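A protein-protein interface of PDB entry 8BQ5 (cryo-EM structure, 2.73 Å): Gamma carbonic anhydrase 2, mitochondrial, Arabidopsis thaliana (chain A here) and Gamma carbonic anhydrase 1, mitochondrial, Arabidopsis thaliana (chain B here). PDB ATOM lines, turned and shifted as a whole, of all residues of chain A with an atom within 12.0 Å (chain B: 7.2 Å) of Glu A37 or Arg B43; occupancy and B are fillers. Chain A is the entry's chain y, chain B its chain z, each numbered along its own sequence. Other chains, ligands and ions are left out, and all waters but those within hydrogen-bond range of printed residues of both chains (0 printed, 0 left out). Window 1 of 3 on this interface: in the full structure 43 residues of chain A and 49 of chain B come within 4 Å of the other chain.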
ATOM      1  N   ASP A  23      -4.680  38.243  16.176  1.00  0.00           N
ATOM      2  CA  ASP A  23      -4.674  36.855  16.623  1.00  0.00           C
ATOM      3  C   ASP A  23      -5.981  36.162  16.262  1.00  0.00           C
ATOM      4  O   ASP A  23      -5.981  35.021  15.784  1.00  0.00           O
ATOM      5  CB  ASP A  23      -4.427  36.803  18.130  1.00  0.00           C
ATOM      6  CG  ASP A  23      -4.038  35.421  18.618  1.00  0.00           C
ATOM      7  OD1 ASP A  23      -3.453  34.648  17.835  1.00  0.00           O
ATOM      8  OD2 ASP A  23      -4.308  35.113  19.797  1.00  0.00           O
ATOM      9  N   SER A  27      -6.593  33.030  13.736  1.00  0.00           N
ATOM     10  CA  SER A  27      -7.325  31.843  14.169  1.00  0.00           C
ATOM     11  C   SER A  27      -8.433  31.494  13.185  1.00  0.00           C
ATOM     12  O   SER A  27      -8.659  30.318  12.880  1.00  0.00           O
ATOM     13  CB  SER A  27      -7.909  32.061  15.565  1.00  0.00           C
ATOM     14  OG  SER A  27      -6.890  32.273  16.522  1.00  0.00           O
ATOM     15  N   GLN A  30      -7.037  29.842  10.212  1.00  0.00           N
ATOM     16  CA  GLN A  30      -6.625  28.443  10.515  1.00  0.00           C
ATOM     17  C   GLN A  30      -7.828  27.517  10.354  1.00  0.00           C
ATOM     18  O   GLN A  30      -7.616  26.300  10.274  1.00  0.00           O
ATOM     19  CB  GLN A  30      -6.055  28.331  11.928  1.00  0.00           C
ATOM     20  CG  GLN A  30      -4.666  28.920  12.079  1.00  0.00           C
ATOM     21  CD  GLN A  30      -3.981  28.341  13.289  1.00  0.00           C
ATOM     22  OE1 GLN A  30      -4.449  28.472  14.415  1.00  0.00           O
ATOM     23  NE2 GLN A  30      -2.865  27.678  13.056  1.00  0.00           N
ATOM     24  N   SER A  32     -10.556  27.544  12.507  1.00  0.00           N
ATOM     25  CA  SER A  32     -11.058  27.200  13.865  1.00  0.00           C
ATOM     26  C   SER A  32     -10.672  25.760  14.247  1.00  0.00           C
ATOM     27  O   SER A  32     -11.312  25.212  15.164  1.00  0.00           O
ATOM     28  CB  SER A  32     -12.542  27.449  13.982  1.00  0.00           C
ATOM     29  OG  SER A  32     -12.893  28.726  13.466  1.00  0.00           O
ATOM     30  N   HIS A  33      -9.645  25.189  13.612  1.00  0.00           N
ATOM     31  CA  HIS A  33      -9.249  23.776  13.861  1.00  0.00           C
ATOM     32  C   HIS A  33      -8.427  23.678  15.147  1.00  0.00           C
ATOM     33  O   HIS A  33      -8.659  22.724  15.909  1.00  0.00           O
ATOM     34  CB  HIS A  33      -8.465  23.214  12.672  1.00  0.00           C
ATOM     35  CG  HIS A  33      -9.304  22.683  11.561  1.00  0.00           C
ATOM     36  ND1 HIS A  33     -10.679  22.785  11.550  1.00  0.00           N
ATOM     37  CD2 HIS A  33      -8.961  22.047  10.421  1.00  0.00           C
ATOM     38  CE1 HIS A  33     -11.149  22.233  10.452  1.00  0.00           C
ATOM     39  NE2 HIS A  33     -10.115  21.767   9.745  1.00  0.00           N
ATOM     40  N   ARG A  34      -7.526  24.639  15.378  1.00  0.00           N
ATOM     41  CA  ARG A  34      -6.639  24.573  16.566  1.00  0.00           C
ATOM     42  C   ARG A  34      -7.460  24.682  17.843  1.00  0.00           C
ATOM     43  O   ARG A  34      -8.228  25.643  17.974  1.00  0.00           O
ATOM     44  CB  ARG A  34      -5.547  25.644  16.559  1.00  0.00           C
ATOM     45  CG  ARG A  34      -4.372  25.258  17.445  1.00  0.00           C
ATOM     46  CD  ARG A  34      -3.310  26.313  17.657  1.00  0.00           C
ATOM     47  NE  ARG A  34      -2.253  25.770  18.497  1.00  0.00           N
ATOM     48  CZ  ARG A  34      -2.193  25.897  19.817  1.00  0.00           C
ATOM     49  NH1 ARG A  34      -3.126  26.572  20.466  1.00  0.00           N
ATOM     50  NH2 ARG A  34      -1.191  25.356  20.484  1.00  0.00           N
ATOM     51  N   ILE A  35      -7.307  23.703  18.734  1.00  0.00           N
ATOM     52  CA  ILE A  35      -7.989  23.771  20.058  1.00  0.00           C
ATOM     53  C   ILE A  35      -7.177  24.735  20.924  1.00  0.00           C
ATOM     54  O   ILE A  35      -5.952  24.650  20.925  1.00  0.00           O
ATOM     55  CB  ILE A  35      -8.161  22.371  20.679  1.00  0.00           C
ATOM     56  CG1 ILE A  35      -9.161  21.539  19.872  1.00  0.00           C
ATOM     57  CG2 ILE A  35      -8.562  22.457  22.142  1.00  0.00           C
ATOM     58  CD1 ILE A  35      -8.847  20.069  19.812  1.00  0.00           C
ATOM     59  N   GLU A  36      -7.842  25.669  21.580  1.00  0.00           N
ATOM     60  CA  GLU A  36      -7.148  26.675  22.369  1.00  0.00           C
ATOM     61  C   GLU A  36      -6.695  26.102  23.703  1.00  0.00           C
ATOM     62  O   GLU A  36      -7.409  25.322  24.336  1.00  0.00           O
ATOM     63  CB  GLU A  36      -8.053  27.884  22.604  1.00  0.00           C
ATOM     64  CG  GLU A  36      -8.360  28.674  21.347  1.00  0.00           C
ATOM     65  CD  GLU A  36      -7.737  30.054  21.358  1.00  0.00           C
ATOM     66  OE1 GLU A  36      -6.497  30.146  21.475  1.00  0.00           O
ATOM     67  OE2 GLU A  36      -8.486  31.048  21.243  1.00  0.00           O
ATOM     68  N   GLU A  37      -5.492  26.483  24.119  1.00  0.00           N
ATOM     69  CA  GLU A  37      -5.039  26.182  25.467  1.00  0.00           C
ATOM     70  C   GLU A  37      -5.830  27.010  26.476  1.00  0.00           C
ATOM     71  O   GLU A  37      -6.187  28.164  26.222  1.00  0.00           O
ATOM     72  CB  GLU A  37      -3.540  26.458  25.598  1.00  0.00           C
ATOM     73  CG  GLU A  37      -2.668  25.583  24.711  1.00  0.00           C
ATOM     74  CD  GLU A  37      -1.407  26.283  24.245  1.00  0.00           C
ATOM     75  OE1 GLU A  37      -1.240  26.462  23.021  1.00  0.00           O
ATOM     76  OE2 GLU A  37      -0.579  26.651  25.103  1.00  0.00           O
ATOM     77  N   HIS A  38      -6.104  26.412  27.634  1.00  0.00           N
ATOM     78  CA  HIS A  38      -6.947  27.038  28.644  1.00  0.00           C
ATOM     79  C   HIS A  38      -6.248  27.011  29.996  1.00  0.00           C
ATOM     80  O   HIS A  38      -5.192  26.396  30.166  1.00  0.00           O
ATOM     81  CB  HIS A  38      -8.310  26.344  28.761  1.00  0.00           C
ATOM     82  CG  HIS A  38      -9.168  26.475  27.542  1.00  0.00           C
ATOM     83  ND1 HIS A  38      -9.995  27.555  27.326  1.00  0.00           N
ATOM     84  CD2 HIS A  38      -9.346  25.647  26.485  1.00  0.00           C
ATOM     85  CE1 HIS A  38     -10.636  27.395  26.182  1.00  0.00           C
ATOM     86  NE2 HIS A  38     -10.259  26.245  25.651  1.00  0.00           N
ATOM     87  N   LEU A  39      -6.861  27.687  30.966  1.00  0.00           N
ATOM     88  CA  LEU A  39      -6.375  27.639  32.338  1.00  0.00           C
ATOM     89  C   LEU A  39      -6.417  26.210  32.863  1.00  0.00           C
ATOM     90  O   LEU A  39      -7.341  25.448  32.567  1.00  0.00           O
ATOM     91  CB  LEU A  39      -7.218  28.551  33.229  1.00  0.00           C
ATOM     92  CG  LEU A  39      -6.511  29.114  34.458  1.00  0.00           C
ATOM     93  CD1 LEU A  39      -5.223  29.806  34.058  1.00  0.00           C
ATOM     94  CD2 LEU A  39      -7.425  30.067  35.205  1.00  0.00           C
ATOM     95  N   SER A  40      -5.402  25.847  33.643  1.00  0.00           N
ATOM     96  CA  SER A  40      -5.266  24.473  34.108  1.00  0.00           C
ATOM     97  C   SER A  40      -6.401  24.108  35.057  1.00  0.00           C
ATOM     98  O   SER A  40      -6.675  24.824  36.024  1.00  0.00           O
ATOM     99  CB  SER A  40      -3.919  24.281  34.800  1.00  0.00           C
ATOM    100  OG  SER A  40      -3.789  22.965  35.306  1.00  0.00           O
ATOM    101  N   ARG A  41      -7.051  22.972  34.785  1.00  0.00           N
ATOM    102  CA  ARG A  41      -8.167  22.495  35.645  1.00  0.00           C
ATOM    103  C   ARG A  41      -7.737  21.266  36.455  1.00  0.00           C
ATOM    104  O   ARG A  41      -8.607  20.655  37.090  1.00  0.00           O
ATOM    105  CB  ARG A  41      -9.368  22.131  34.774  1.00  0.00           C
ATOM    106  CG  ARG A  41     -10.068  23.332  34.155  1.00  0.00           C
ATOM    107  CD  ARG A  41     -11.482  23.010  33.719  1.00  0.00           C
ATOM    108  NE  ARG A  41     -12.351  22.700  34.845  1.00  0.00           N
ATOM    109  CZ  ARG A  41     -13.116  23.581  35.480  1.00  0.00           C
ATOM    110  NH1 ARG A  41     -13.128  24.846  35.098  1.00  0.00           N
ATOM    111  NH2 ARG A  41     -13.868  23.193  36.493  1.00  0.00           N
ATOM    112  N   HIS A  42      -6.448  20.932  36.452  1.00  0.00           N
ATOM    113  CA  HIS A  42      -5.959  19.797  37.276  1.00  0.00           C
ATOM    114  C   HIS A  42      -6.026  20.148  38.766  1.00  0.00           C
ATOM    115  O   HIS A  42      -5.539  21.225  39.137  1.00  0.00           O
ATOM    116  CB  HIS A  42      -4.545  19.376  36.871  1.00  0.00           C
ATOM    117  CG  HIS A  42      -3.986  18.337  37.782  1.00  0.00           C
ATOM    118  ND1 HIS A  42      -4.551  17.085  37.906  1.00  0.00           N
ATOM    119  CD2 HIS A  42      -2.955  18.375  38.649  1.00  0.00           C
ATOM    120  CE1 HIS A  42      -3.873  16.389  38.791  1.00  0.00           C
ATOM    121  NE2 HIS A  42      -2.892  17.156  39.258  1.00  0.00           N
ATOM    122  N   TYR B   9      -3.681  26.872   7.460  1.00  0.00           N
ATOM    123  CA  TYR B   9      -3.376  26.663   8.898  1.00  0.00           C
ATOM    124  C   TYR B   9      -2.004  27.273   9.212  1.00  0.00           C
ATOM    125  O   TYR B   9      -1.876  27.939  10.246  1.00  0.00           O
ATOM    126  CB  TYR B   9      -3.461  25.164   9.185  1.00  0.00           C
ATOM    127  CG  TYR B   9      -3.510  24.753  10.634  1.00  0.00           C
ATOM    128  CD1 TYR B   9      -4.691  24.814  11.354  1.00  0.00           C
ATOM    129  CD2 TYR B   9      -2.387  24.254  11.272  1.00  0.00           C
ATOM    130  CE1 TYR B   9      -4.747  24.421  12.680  1.00  0.00           C
ATOM    131  CE2 TYR B   9      -2.427  23.852  12.595  1.00  0.00           C
ATOM    132  CZ  TYR B   9      -3.611  23.939  13.301  1.00  0.00           C
ATOM    133  OH  TYR B   9      -3.655  23.545  14.605  1.00  0.00           O
ATOM    134  N   ARG B  16      -1.231  34.898  13.638  1.00  0.00           N
ATOM    135  CA  ARG B  16      -1.427  34.755  15.103  1.00  0.00           C
ATOM    136  C   ARG B  16      -0.139  35.122  15.849  1.00  0.00           C
ATOM    137  O   ARG B  16      -0.228  35.914  16.785  1.00  0.00           O
ATOM    138  CB  ARG B  16      -1.842  33.332  15.469  1.00  0.00           C
ATOM    139  CG  ARG B  16      -3.223  32.937  14.974  1.00  0.00           C
ATOM    140  CD  ARG B  16      -3.650  31.608  15.558  1.00  0.00           C
ATOM    141  NE  ARG B  16      -3.871  31.737  16.989  1.00  0.00           N
ATOM    142  CZ  ARG B  16      -4.329  30.773  17.775  1.00  0.00           C
ATOM    143  NH1 ARG B  16      -4.630  29.590  17.269  1.00  0.00           N
ATOM    144  NH2 ARG B  16      -4.494  30.999  19.064  1.00  0.00           N
ATOM    145  N   LEU B  39       3.132  28.947  32.421  1.00  0.00           N
ATOM    146  CA  LEU B  39       1.861  28.281  32.651  1.00  0.00           C
ATOM    147  C   LEU B  39       1.776  27.046  31.767  1.00  0.00           C
ATOM    148  O   LEU B  39       2.320  27.026  30.660  1.00  0.00           O
ATOM    149  CB  LEU B  39       0.685  29.218  32.369  1.00  0.00           C
ATOM    150  CG  LEU B  39       0.664  30.516  33.176  1.00  0.00           C
ATOM    151  CD1 LEU B  39       0.059  31.648  32.363  1.00  0.00           C
ATOM    152  CD2 LEU B  39      -0.091  30.321  34.475  1.00  0.00           C
ATOM    153  N   SER B  40       1.099  26.016  32.265  1.00  0.00           N
ATOM    154  CA  SER B  40       1.072  24.740  31.563  1.00  0.00           C
ATOM    155  C   SER B  40       0.317  24.859  30.247  1.00  0.00           C
ATOM    156  O   SER B  40      -0.811  25.356  30.201  1.00  0.00           O
ATOM    157  CB  SER B  40       0.434  23.666  32.437  1.00  0.00           C
ATOM    158  OG  SER B  40       0.344  22.444  31.729  1.00  0.00           O
ATOM    159  N   ARG B  41       0.945  24.380  29.177  1.00  0.00           N
ATOM    160  CA  ARG B  41       0.357  24.363  27.847  1.00  0.00           C
ATOM    161  C   ARG B  41      -0.338  23.041  27.549  1.00  0.00           C
ATOM    162  O   ARG B  41      -0.656  22.765  26.388  1.00  0.00           O
ATOM    163  CB  ARG B  41       1.438  24.654  26.803  1.00  0.00           C
ATOM    164  CG  ARG B  41       2.430  25.707  27.276  1.00  0.00           C
ATOM    165  CD  ARG B  41       3.115  26.483  26.158  1.00  0.00           C
ATOM    166  NE  ARG B  41       2.291  26.712  24.979  1.00  0.00           N
ATOM    167  CZ  ARG B  41       2.731  27.299  23.875  1.00  0.00           C
ATOM    168  NH1 ARG B  41       3.969  27.756  23.785  1.00  0.00           N
ATOM    169  NH2 ARG B  41       1.911  27.437  22.838  1.00  0.00           N
ATOM    170  N   HIS B  42      -0.568  22.218  28.570  1.00  0.00           N
ATOM    171  CA  HIS B  42      -1.228  20.935  28.374  1.00  0.00           C
ATOM    172  C   HIS B  42      -2.678  21.132  27.959  1.00  0.00           C
ATOM    173  O   HIS B  42      -3.403  21.940  28.545  1.00  0.00           O
ATOM    174  CB  HIS B  42      -1.168  20.101  29.656  1.00  0.00           C
ATOM    175  CG  HIS B  42      -2.137  18.960  29.675  1.00  0.00           C
ATOM    176  ND1 HIS B  42      -1.942  17.807  28.946  1.00  0.00           N
ATOM    177  CD2 HIS B  42      -3.318  18.803  30.317  1.00  0.00           C
ATOM    178  CE1 HIS B  42      -2.956  16.984  29.148  1.00  0.00           C
ATOM    179  NE2 HIS B  42      -3.804  17.565  29.977  1.00  0.00           N
ATOM    180  N   ARG B  43      -3.102  20.375  26.957  1.00  0.00           N
ATOM    181  CA  ARG B  43      -4.483  20.375  26.502  1.00  0.00           C
ATOM    182  C   ARG B  43      -5.042  18.969  26.649  1.00  0.00           C
ATOM    183  O   ARG B  43      -4.434  18.004  26.177  1.00  0.00           O
ATOM    184  CB  ARG B  43      -4.584  20.852  25.052  1.00  0.00           C
ATOM    185  CG  ARG B  43      -4.600  22.364  24.913  1.00  0.00           C
ATOM    186  CD  ARG B  43      -4.576  22.801  23.462  1.00  0.00           C
ATOM    187  NE  ARG B  43      -3.328  22.447  22.795  1.00  0.00           N
ATOM    188  CZ  ARG B  43      -3.150  22.470  21.482  1.00  0.00           C
ATOM    189  NH1 ARG B  43      -4.122  22.828  20.659  1.00  0.00           N
ATOM    190  NH2 ARG B  43      -1.966  22.130  20.982  1.00  0.00           N
ATOM    191  N   THR B  44      -6.191  18.858  27.318  1.00  0.00           N
ATOM    192  CA  THR B  44      -6.840  17.560  27.457  1.00  0.00           C
ATOM    193  C   THR B  44      -7.183  16.981  26.092  1.00  0.00           C
ATOM    194  O   THR B  44      -6.948  15.795  25.832  1.00  0.00           O
ATOM    195  CB  THR B  44      -8.097  17.694  28.317  1.00  0.00           C
ATOM    196  OG1 THR B  44      -7.773  18.372  29.536  1.00  0.00           O
ATOM    197  CG2 THR B  44      -8.671  16.332  28.644  1.00  0.00           C
ATOM    198  N   LEU B  45      -7.720  17.809  25.205  1.00  0.00           N
ATOM    199  CA  LEU B  45      -8.029  17.424  23.837  1.00  0.00           C
ATOM    200  C   LEU B  45      -7.160  18.244  22.896  1.00  0.00           C
ATOM    201  O   LEU B  45      -7.350  19.458  22.775  1.00  0.00           O
ATOM    202  CB  LEU B  45      -9.509  17.654  23.531  1.00  0.00           C
ATOM    203  CG  LEU B  45     -10.538  16.940  24.410  1.00  0.00           C
ATOM    204  CD1 LEU B  45     -11.879  16.888  23.706  1.00  0.00           C
ATOM    205  CD2 LEU B  45     -10.083  15.539  24.778  1.00  0.00           C
ATOM    206  N   MET B  46      -6.206  17.590  22.241  1.00  0.00           N
ATOM    207  CA  MET B  46      -5.289  18.276  21.344  1.00  0.00           C
ATOM    208  C   MET B  46      -5.494  17.782  19.922  1.00  0.00           C
ATOM    209  O   MET B  46      -5.692  16.584  19.697  1.00  0.00           O
ATOM    210  CB  MET B  46      -3.828  18.080  21.761  1.00  0.00           C
ATOM    211  CG  MET B  46      -2.888  19.006  21.004  1.00  0.00           C
ATOM    212  SD  MET B  46      -1.281  18.317  20.578  1.00  0.00           S
ATOM    213  CE  MET B  46      -0.603  18.040  22.204  1.00  0.00           C
ATOM    214  N   ASN B  47      -5.436  18.737  19.000  1.00  0.00           N
ATOM    215  CA  ASN B  47      -5.579  18.422  17.563  1.00  0.00           C
ATOM    216  C   ASN B  47      -4.238  18.427  16.837  1.00  0.00           C
ATOM    217  O   ASN B  47      -3.331  19.175  17.240  1.00  0.00           O
ATOM    218  CB  ASN B  47      -6.479  19.443  16.868  1.00  0.00           C
ATOM    219  CG  ASN B  47      -5.886  20.834  16.828  1.00  0.00           C
ATOM    220  OD1 ASN B  47      -5.720  21.472  17.863  1.00  0.00           O
ATOM    221  ND2 ASN B  47      -5.539  21.303  15.642  1.00  0.00           N
ATOM    222  N   VAL B  48      -4.096  17.574  15.837  1.00  0.00           N
ATOM    223  CA  VAL B  48      -2.943  17.592  14.946  1.00  0.00           C
ATOM    224  C   VAL B  48      -3.477  18.028  13.588  1.00  0.00           C
ATOM    225  O   VAL B  48      -3.903  17.193  12.781  1.00  0.00           O
ATOM    226  CB  VAL B  48      -2.239  16.234  14.870  1.00  0.00           C
ATOM    227  CG1 VAL B  48      -1.032  16.315  13.948  1.00  0.00           C
ATOM    228  CG2 VAL B  48      -1.826  15.771  16.257  1.00  0.00           C
ATOM    229  N   PRO B  63      -9.045  15.750  33.554  1.00  0.00           N
ATOM    230  CA  PRO B  63      -8.343  16.917  32.991  1.00  0.00           C
ATOM    231  C   PRO B  63      -6.883  16.653  32.669  1.00  0.00           C
ATOM    232  O   PRO B  63      -6.346  17.254  31.732  1.00  0.00           O
ATOM    233  CB  PRO B  63      -8.509  17.983  34.084  1.00  0.00           C
ATOM    234  CG  PRO B  63      -9.708  17.559  34.854  1.00  0.00           C
ATOM    235  CD  PRO B  63      -9.711  16.062  34.830  1.00  0.00           C
ATOM    236  N   SER B  64      -6.226  15.759  33.409  1.00  0.00           N
ATOM    237  CA  SER B  64      -4.821  15.453  33.168  1.00  0.00           C
ATOM    238  C   SER B  64      -4.608  14.413  32.074  1.00  0.00           C
ATOM    239  O   SER B  64      -3.456  14.141  31.724  1.00  0.00           O
ATOM    240  CB  SER B  64      -4.158  14.978  34.464  1.00  0.00           C
ATOM    241  OG  SER B  64      -4.719  13.759  34.916  1.00  0.00           O
ATOM    242  N   ALA B  65      -5.672  13.831  31.528  1.00  0.00           N
ATOM    243  CA  ALA B  65      -5.523  12.880  30.437  1.00  0.00           C
ATOM    244  C   ALA B  65      -5.101  13.593  29.155  1.00  0.00           C
ATOM    245  O   ALA B  65      -5.348  14.787  28.971  1.00  0.00           O
ATOM    246  CB  ALA B  65      -6.829  12.119  30.207  1.00  0.00           C
ATOM    247  N   SER B  66      -4.448  12.847  28.268  1.00  0.00           N
ATOM    248  CA  SER B  66      -3.985  13.363  26.986  1.00  0.00           C
ATOM    249  C   SER B  66      -4.677  12.600  25.867  1.00  0.00           C
ATOM    250  O   SER B  66      -4.433  11.403  25.682  1.00  0.00           O
ATOM    251  CB  SER B  66      -2.466  13.238  26.853  1.00  0.00           C
ATOM    252  OG  SER B  66      -1.794  13.974  27.857  1.00  0.00           O
ATOM    253  N   VAL B  67      -5.532  13.292  25.123  1.00  0.00           N
ATOM    254  CA  VAL B  67      -6.228  12.722  23.978  1.00  0.00           C
ATOM    255  C   VAL B  67      -5.767  13.497  22.752  1.00  0.00           C
ATOM    256  O   VAL B  67      -6.082  14.684  22.603  1.00  0.00           O
ATOM    257  CB  VAL B  67      -7.752  12.786  24.146  1.00  0.00           C
ATOM    258  CG1 VAL B  67      -8.432  12.011  23.050  1.00  0.00           C
ATOM    259  CG2 VAL B  67      -8.153  12.235  25.506  1.00  0.00           C
ATOM    260  N   ILE B  68      -5.029  12.829  21.870  1.00  0.00           N
ATOM    261  CA  ILE B  68      -4.332  13.477  20.768  1.00  0.00           C
ATOM    262  C   ILE B  68      -4.834  12.904  19.451  1.00  0.00           C
ATOM    263  O   ILE B  68      -4.832  11.684  19.259  1.00  0.00           O
ATOM    264  CB  ILE B  68      -2.808  13.295  20.880  1.00  0.00           C
ATOM    265  CG1 ILE B  68      -2.300  13.819  22.221  1.00  0.00           C
ATOM    266  CG2 ILE B  68      -2.119  13.992  19.732  1.00  0.00           C
ATOM    267  CD1 ILE B  68      -1.821  12.729  23.161  1.00  0.00           C
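The side-chain carboxylate (OD1) of Asp A23 lies within salt-bridge range of the guanidinium group (NE) of Arg B16 (3.1 Å). OG of Ser A27 sits at hydrogen-bond distance from NE of Arg B16. O of Tyr B9 sits at hydrogen-bond distance from NE2 of Gln A30. The guanidinium group (NH1) of Arg B16 sits at hydrogen-bond distance from the side-chain amide oxygen (OE1) of Gln A30 (3.1 Å). The backbone carbonyl oxygen of His A33 lies within hydrogen-bond range of the side-chain amide nitrogen of Asn B47 (3.4 Å). The backbone carbonyl oxygen (O) of Ile A35 is in hydrogen-bond range of the guanidinium group (NH1) of Arg B43, at 2.6 Å. The backbone NH (N) of Ile A35 lies within hydrogen-bond range of the side-chain amide oxygen (OD1) of Asn B47, at 2.9 Å. The side-chain carboxylate of Glu A36 lies within salt-bridge range of the guanidinium group of Arg B16, at 3.2 Å. OE2 of Glu A37 lies within salt-bridge range of NE of Arg B41 (2.9 Å). NH2 of Arg B43 lies close to NH2 of Arg A34 (3.4 Å).
Of the 18 printed residues of chain B, 7 touch a printed residue of chain A. Hydrophobic or aromatic side chains of chain B within 4 Å of the printed part of chain A: Tyr B9 and Pro B63. Of the 14 printed residues of chain A, 9 touch a printed residue of chain B. Among the printed residues, 18 pairs touch across the chains. Among the printed residues, Asp or Glu carboxylates within 4 Å of a Lys or Arg side-chain nitrogen of the other chain: Asp A23 with Arg B16, Glu A36 with Arg B16 and Glu A37 with Arg B41.
Printed residues of chain B within 4 Å of Glu A37: Arg B41 and Arg B43. Arg B43 touches just these residues of chain A: Arg A34, Ile A35, Glu A36 and Glu A37. Arg B41 touches just one residue of chain A: Glu A37. No residue of chain A comes within 4 Å of His B42. No residue of chain A comes within 4 Å of Thr B44. No residue of chain A comes within 4 Å of Met B46. Asn B47 touches just these residues of chain A: His A33 (3.4 Å), Arg A34 (3.5 Å) and Ile A35 (2.9 Å). Ala B65 touches none of the printed residues of chain A. No residue of chain A comes within 4 Å of Val B67. Of the printed residues of chain A, Arg B16 touches Asp A23 (3.1 Å), Ser A27 (3.1 Å), Gln A30 (3.1 Å), Arg A34 (3.6 Å) and Glu A36 (3.2 Å). Of the printed residues of chain A, Tyr B9 touches Gln A30, His A33 and Arg A34. Printed residues of chain B within 4 Å of Ile A35: Arg B43 (2.6 Å), Leu B45 (3.3 Å) and Asn B47 (2.9 Å). His A38 touches none of the printed residues of chain B. The nearest residue of chain B that does not touch Glu A37 is Ser B40 (5.3 Å). The nearest residue of chain A that does not touch Arg B43 is His A38 (5.1 Å). The nearest printed residue of chain B that does not touch Arg A41 is Ser B64 (6.5 Å).
Among the printed residues, merely in contact across the chains: Ile A35 with Leu B45 (3.3 Å), Arg A34 with Tyr B9 (3.4 Å), Arg A34 with Asn B47 (3.5 Å), Arg A34 with Arg B16 (3.6 Å), Glu A37 with Arg B43 (3.6 Å), Glu A36 with Arg B43 (3.9 Å), His A33 with Tyr B9 (3.9 Å) and Arg A41 with Pro B63 (3.97 Å).
OG of Ser A27 sits at hydrogen-bond distance from O of Asp A23 (3.0 Å). NH2 of Arg A34 lies within salt-bridge range of OE1 of Glu A37 (2.8 Å). NE2 of His A38 lies close to O of Glu A36 (3.3 Å). The side-chain amide nitrogen (ND2) of Asn B47 is in hydrogen-bond range of the side-chain hydroxyl (OH) of Tyr B9 (3.1 Å). A ring nitrogen (NE2) of His B42 is in hydrogen-bond range of the backbone carbonyl oxygen of Pro B63. The backbone carbonyl oxygen (O) of Pro B63 lies within hydrogen-bond range of the side-chain hydroxyl (OG1) of Thr B44, at 2.8 Å.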
